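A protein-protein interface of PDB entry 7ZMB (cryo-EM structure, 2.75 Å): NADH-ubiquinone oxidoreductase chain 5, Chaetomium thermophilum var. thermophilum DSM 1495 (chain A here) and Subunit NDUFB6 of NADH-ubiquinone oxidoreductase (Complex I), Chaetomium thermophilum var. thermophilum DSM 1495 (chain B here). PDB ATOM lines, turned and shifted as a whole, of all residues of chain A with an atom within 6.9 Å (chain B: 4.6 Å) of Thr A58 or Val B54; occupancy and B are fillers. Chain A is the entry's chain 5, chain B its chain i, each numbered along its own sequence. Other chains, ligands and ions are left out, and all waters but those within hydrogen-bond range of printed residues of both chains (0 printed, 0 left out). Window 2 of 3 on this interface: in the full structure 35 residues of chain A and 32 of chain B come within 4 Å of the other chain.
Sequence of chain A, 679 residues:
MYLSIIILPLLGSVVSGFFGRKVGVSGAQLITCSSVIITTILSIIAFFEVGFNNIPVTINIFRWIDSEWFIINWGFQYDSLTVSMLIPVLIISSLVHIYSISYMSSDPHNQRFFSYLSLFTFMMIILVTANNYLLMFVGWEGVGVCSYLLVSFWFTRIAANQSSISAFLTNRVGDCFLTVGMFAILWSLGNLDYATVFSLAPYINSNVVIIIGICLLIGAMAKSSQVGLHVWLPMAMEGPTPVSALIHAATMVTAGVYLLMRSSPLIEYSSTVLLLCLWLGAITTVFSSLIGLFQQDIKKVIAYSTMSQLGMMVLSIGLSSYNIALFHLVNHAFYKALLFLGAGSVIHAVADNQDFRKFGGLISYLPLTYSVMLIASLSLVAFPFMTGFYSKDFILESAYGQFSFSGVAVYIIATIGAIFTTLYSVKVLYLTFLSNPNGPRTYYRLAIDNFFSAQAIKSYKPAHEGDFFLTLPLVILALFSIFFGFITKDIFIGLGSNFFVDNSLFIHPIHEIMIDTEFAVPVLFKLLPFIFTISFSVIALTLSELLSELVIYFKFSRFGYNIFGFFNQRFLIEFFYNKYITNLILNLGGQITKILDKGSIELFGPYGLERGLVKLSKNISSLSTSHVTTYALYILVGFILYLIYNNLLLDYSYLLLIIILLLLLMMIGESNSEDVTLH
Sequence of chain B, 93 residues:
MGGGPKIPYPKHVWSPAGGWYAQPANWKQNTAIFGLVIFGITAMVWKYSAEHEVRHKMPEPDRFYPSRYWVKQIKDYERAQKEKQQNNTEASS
The backbone carbonyl oxygen (O) of Val B54 lies within hydrogen-bond range of the backbone NH (N) of Thr A58, 3.4 Å away.
Of the 5 printed residues of chain B, 4 touch a printed residue of chain A. Among the printed residues, 8 pairs touch across the chains.
CG2 of Ile A55 touches CG of Arg B55 (3.7 Å). Val B54 touches Val A57 (O to CA, 3.9 Å). Val A57 touches Arg B55 (CG1 to NE, 3.2 Å). Thr A58 touches His B52. Thr A58 touches Glu B53 (O to CA, 3.96 Å). Ile A59 touches His B52. Ile A59 touches Glu B53.
The side-chain carboxylate (OE1) of Glu B53 lies within salt-bridge range of the guanidinium group (NH1) of Arg B55 (3.0 Å). O of Val A57 sits close to OE1 of Gln A77, 3.4 Å away. The backbone NH (N) of Tyr A78 sits at hydrogen-bond distance from the backbone carbonyl oxygen (O) of Val A57, at 2.9 Å. The backbone NH of Phe A76 is in hydrogen-bond range of the backbone carbonyl oxygen of Ile A59 (2.5 Å).
Printed residues of chain B within 4 Å of Val A57: Val B54 and Arg B55. Thr A58 touches just these residues of chain B: His B52, Glu B53 and Val B54. Phe A76 touches none of the printed residues of chain B. Tyr A78 touches none of the printed residues of chain B. Of the printed residues of chain A, Glu B53 touches Thr A58 and Ile A59. Printed residues of chain A within 4 Å of Arg B55: Ile A55 (3.7 Å) and Val A57 (3.2 Å). The nearest printed residue of chain B that does not touch Thr A58 is Arg B55 (5.6 Å). The nearest residue of chain A that does not touch Val B54 is Pro A56 (4.4 Å).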
ATOM      1  N   ILE A  55      23.014 -15.465  18.266  1.00  0.00           N
ATOM      2  CA  ILE A  55      22.642 -16.520  17.323  1.00  0.00           C
ATOM      3  C   ILE A  55      23.621 -17.676  17.441  1.00  0.00           C
ATOM      4  O   ILE A  55      24.732 -17.607  16.896  1.00  0.00           O
ATOM      5  CB  ILE A  55      22.580 -16.036  15.866  1.00  0.00           C
ATOM      6  CG1 ILE A  55      21.507 -14.977  15.660  1.00  0.00           C
ATOM      7  CG2 ILE A  55      22.322 -17.197  14.943  1.00  0.00           C
ATOM      8  CD1 ILE A  55      21.956 -13.599  15.879  1.00  0.00           C
ATOM      9  N   PRO A  56      23.262 -18.744  18.140  1.00  0.00           N
ATOM     10  CA  PRO A  56      24.047 -19.972  18.060  1.00  0.00           C
ATOM     11  C   PRO A  56      23.766 -20.713  16.762  1.00  0.00           C
ATOM     12  O   PRO A  56      22.640 -20.734  16.260  1.00  0.00           O
ATOM     13  CB  PRO A  56      23.577 -20.765  19.284  1.00  0.00           C
ATOM     14  CG  PRO A  56      22.212 -20.302  19.521  1.00  0.00           C
ATOM     15  CD  PRO A  56      22.121 -18.875  19.056  1.00  0.00           C
ATOM     16  N   VAL A  57      24.812 -21.325  16.213  1.00  0.00           N
ATOM     17  CA  VAL A  57      24.752 -21.954  14.899  1.00  0.00           C
ATOM     18  C   VAL A  57      25.133 -23.423  15.017  1.00  0.00           C
ATOM     19  O   VAL A  57      26.047 -23.782  15.765  1.00  0.00           O
ATOM     20  CB  VAL A  57      25.662 -21.232  13.888  1.00  0.00           C
ATOM     21  CG1 VAL A  57      25.082 -19.887  13.529  1.00  0.00           C
ATOM     22  CG2 VAL A  57      27.027 -21.053  14.467  1.00  0.00           C
ATOM     23  N   THR A  58      24.432 -24.267  14.269  1.00  0.00           N
ATOM     24  CA  THR A  58      24.589 -25.714  14.326  1.00  0.00           C
ATOM     25  C   THR A  58      25.088 -26.237  12.986  1.00  0.00           C
ATOM     26  O   THR A  58      24.594 -25.829  11.931  1.00  0.00           O
ATOM     27  CB  THR A  58      23.264 -26.386  14.685  1.00  0.00           C
ATOM     28  OG1 THR A  58      22.818 -25.919  15.963  1.00  0.00           O
ATOM     29  CG2 THR A  58      23.420 -27.893  14.734  1.00  0.00           C
ATOM     30  N   ILE A  59      26.073 -27.131  13.034  1.00  0.00           N
ATOM     31  CA  ILE A  59      26.566 -27.846  11.865  1.00  0.00           C
ATOM     32  C   ILE A  59      26.562 -29.329  12.192  1.00  0.00           C
ATOM     33  O   ILE A  59      27.142 -29.742  13.199  1.00  0.00           O
ATOM     34  CB  ILE A  59      27.977 -27.397  11.458  1.00  0.00           C
ATOM     35  CG1 ILE A  59      27.990 -25.913  11.117  1.00  0.00           C
ATOM     36  CG2 ILE A  59      28.458 -28.196  10.266  1.00  0.00           C
ATOM     37  CD1 ILE A  59      27.101 -25.581   9.955  1.00  0.00           C
ATOM     38  N   ASN A  60      25.919 -30.126  11.344  1.00  0.00           N
ATOM     39  CA  ASN A  60      25.902 -31.582  11.473  1.00  0.00           C
ATOM     40  C   ASN A  60      26.347 -32.165  10.138  1.00  0.00           C
ATOM     41  O   ASN A  60      25.545 -32.278   9.206  1.00  0.00           O
ATOM     42  CB  ASN A  60      24.516 -32.085  11.865  1.00  0.00           C
ATOM     43  CG  ASN A  60      24.145 -31.720  13.287  1.00  0.00           C
ATOM     44  OD1 ASN A  60      24.933 -31.906  14.215  1.00  0.00           O
ATOM     45  ND2 ASN A  60      22.937 -31.202  13.468  1.00  0.00           N
ATOM     46  N   GLY A  75      29.273 -33.315  14.606  1.00  0.00           N
ATOM     47  CA  GLY A  75      28.449 -32.129  14.579  1.00  0.00           C
ATOM     48  C   GLY A  75      29.030 -31.044  15.459  1.00  0.00           C
ATOM     49  O   GLY A  75      29.680 -31.320  16.466  1.00  0.00           O
ATOM     50  N   PHE A  76      28.789 -29.803  15.072  1.00  0.00           N
ATOM     51  CA  PHE A  76      29.415 -28.675  15.733  1.00  0.00           C
ATOM     52  C   PHE A  76      28.378 -27.619  16.059  1.00  0.00           C
ATOM     53  O   PHE A  76      27.523 -27.298  15.233  1.00  0.00           O
ATOM     54  CB  PHE A  76      30.533 -28.112  14.864  1.00  0.00           C
ATOM     55  CG  PHE A  76      31.610 -29.106  14.580  1.00  0.00           C
ATOM     56  CD1 PHE A  76      32.684 -29.244  15.435  1.00  0.00           C
ATOM     57  CD2 PHE A  76      31.530 -29.935  13.480  1.00  0.00           C
ATOM     58  CE1 PHE A  76      33.665 -30.164  15.182  1.00  0.00           C
ATOM     59  CE2 PHE A  76      32.507 -30.863  13.230  1.00  0.00           C
ATOM     60  CZ  PHE A  76      33.576 -30.977  14.083  1.00  0.00           C
ATOM     61  N   GLN A  77      28.453 -27.100  17.281  1.00  0.00           N
ATOM     62  CA  GLN A  77      27.527 -26.094  17.779  1.00  0.00           C
ATOM     63  C   GLN A  77      28.326 -24.921  18.311  1.00  0.00           C
ATOM     64  O   GLN A  77      29.127 -25.088  19.233  1.00  0.00           O
ATOM     65  CB  GLN A  77      26.638 -26.665  18.885  1.00  0.00           C
ATOM     66  CG  GLN A  77      25.713 -25.661  19.533  1.00  0.00           C
ATOM     67  CD  GLN A  77      24.586 -25.260  18.623  1.00  0.00           C
ATOM     68  OE1 GLN A  77      24.266 -25.969  17.679  1.00  0.00           O
ATOM     69  NE2 GLN A  77      23.962 -24.130  18.912  1.00  0.00           N
ATOM     70  N   TYR A  78      28.115 -23.745  17.735  1.00  0.00           N
ATOM     71  CA  TYR A  78      28.675 -22.513  18.268  1.00  0.00           C
ATOM     72  C   TYR A  78      27.623 -21.823  19.114  1.00  0.00           C
ATOM     73  O   TYR A  78      26.478 -21.678  18.687  1.00  0.00           O
ATOM     74  CB  TYR A  78      29.143 -21.572  17.162  1.00  0.00           C
ATOM     75  CG  TYR A  78      30.300 -22.093  16.373  1.00  0.00           C
ATOM     76  CD1 TYR A  78      30.108 -23.015  15.363  1.00  0.00           C
ATOM     77  CD2 TYR A  78      31.582 -21.665  16.632  1.00  0.00           C
ATOM     78  CE1 TYR A  78      31.156 -23.499  14.638  1.00  0.00           C
ATOM     79  CE2 TYR A  78      32.644 -22.144  15.907  1.00  0.00           C
ATOM     80  CZ  TYR A  78      32.421 -23.062  14.909  1.00  0.00           C
ATOM     81  OH  TYR A  78      33.469 -23.560  14.176  1.00  0.00           O
ATOM     82  N   ASN A 131      29.059 -30.816  19.443  1.00  0.00           N
ATOM     83  CA  ASN A 131      27.688 -30.927  19.926  1.00  0.00           C
ATOM     84  C   ASN A 131      27.586 -31.733  21.206  1.00  0.00           C
ATOM     85  O   ASN A 131      26.614 -31.580  21.954  1.00  0.00           O
ATOM     86  CB  ASN A 131      26.773 -31.607  18.909  1.00  0.00           C
ATOM     87  CG  ASN A 131      26.417 -30.734  17.765  1.00  0.00           C
ATOM     88  OD1 ASN A 131      26.228 -29.534  17.928  1.00  0.00           O
ATOM     89  ND2 ASN A 131      26.231 -31.336  16.602  1.00  0.00           N
ATOM     90  N   HIS B  52      24.634 -25.501   5.164  1.00  0.00           N
ATOM     91  CA  HIS B  52      24.118 -26.345   6.271  1.00  0.00           C
ATOM     92  C   HIS B  52      24.071 -25.547   7.565  1.00  0.00           C
ATOM     93  O   HIS B  52      23.602 -26.102   8.571  1.00  0.00           O
ATOM     94  CB  HIS B  52      25.019 -27.563   6.446  1.00  0.00           C
ATOM     95  CG  HIS B  52      24.604 -28.722   5.612  1.00  0.00           C
ATOM     96  ND1 HIS B  52      24.831 -28.765   4.256  1.00  0.00           N
ATOM     97  CD2 HIS B  52      23.973 -29.871   5.936  1.00  0.00           C
ATOM     98  CE1 HIS B  52      24.356 -29.893   3.778  1.00  0.00           C
ATOM     99  NE2 HIS B  52      23.829 -30.591   4.785  1.00  0.00           N
ATOM    100  N   GLU B  53      24.562 -24.310   7.541  1.00  0.00           N
ATOM    101  CA  GLU B  53      24.461 -23.485   8.743  1.00  0.00           C
ATOM    102  C   GLU B  53      22.990 -23.240   9.044  1.00  0.00           C
ATOM    103  O   GLU B  53      22.316 -22.486   8.342  1.00  0.00           O
ATOM    104  CB  GLU B  53      25.207 -22.167   8.561  1.00  0.00           C
ATOM    105  CG  GLU B  53      26.679 -22.222   8.928  1.00  0.00           C
ATOM    106  CD  GLU B  53      27.431 -20.968   8.530  1.00  0.00           C
ATOM    107  OE1 GLU B  53      26.778 -19.929   8.297  1.00  0.00           O
ATOM    108  OE2 GLU B  53      28.677 -21.021   8.448  1.00  0.00           O
ATOM    109  N   VAL B  54      22.484 -23.877  10.095  1.00  0.00           N
ATOM    110  CA  VAL B  54      21.079 -23.787  10.472  1.00  0.00           C
ATOM    111  C   VAL B  54      20.956 -22.923  11.718  1.00  0.00           C
ATOM    112  O   VAL B  54      21.752 -23.045  12.656  1.00  0.00           O
ATOM    113  CB  VAL B  54      20.462 -25.181  10.697  1.00  0.00           C
ATOM    114  CG1 VAL B  54      20.385 -25.935   9.381  1.00  0.00           C
ATOM    115  CG2 VAL B  54      21.280 -25.968  11.702  1.00  0.00           C
ATOM    116  N   ARG B  55      19.966 -22.035  11.714  1.00  0.00           N
ATOM    117  CA  ARG B  55      19.728 -21.109  12.808  1.00  0.00           C
ATOM    118  C   ARG B  55      18.240 -21.071  13.127  1.00  0.00           C
ATOM    119  O   ARG B  55      17.413 -21.655  12.424  1.00  0.00           O
ATOM    120  CB  ARG B  55      20.237 -19.704  12.468  1.00  0.00           C
ATOM    121  CG  ARG B  55      21.731 -19.641  12.239  1.00  0.00           C
ATOM    122  CD  ARG B  55      22.115 -18.514  11.304  1.00  0.00           C
ATOM    123  NE  ARG B  55      23.556 -18.480  11.089  1.00  0.00           N
ATOM    124  CZ  ARG B  55      24.153 -17.802  10.116  1.00  0.00           C
ATOM    125  NH1 ARG B  55      25.473 -17.828  10.001  1.00  0.00           N
ATOM    126  NH2 ARG B  55      23.430 -17.091   9.263  1.00  0.00           N
ATOM    127  N   GLN B  73      20.322 -19.897   4.839  1.00  0.00           N
ATOM    128  CA  GLN B  73      19.165 -19.976   5.722  1.00  0.00           C
ATOM    129  C   GLN B  73      18.521 -18.621   5.975  1.00  0.00           C
ATOM    130  O   GLN B  73      17.348 -18.571   6.358  1.00  0.00           O
ATOM    131  CB  GLN B  73      19.563 -20.615   7.053  1.00  0.00           C
ATOM    132  CG  GLN B  73      18.468 -21.456   7.686  1.00  0.00           C
ATOM    133  CD  GLN B  73      17.603 -20.660   8.639  1.00  0.00           C
ATOM    134  OE1 GLN B  73      18.102 -19.856   9.423  1.00  0.00           O
ATOM    135  NE2 GLN B  73      16.295 -20.879   8.573  1.00  0.00           N
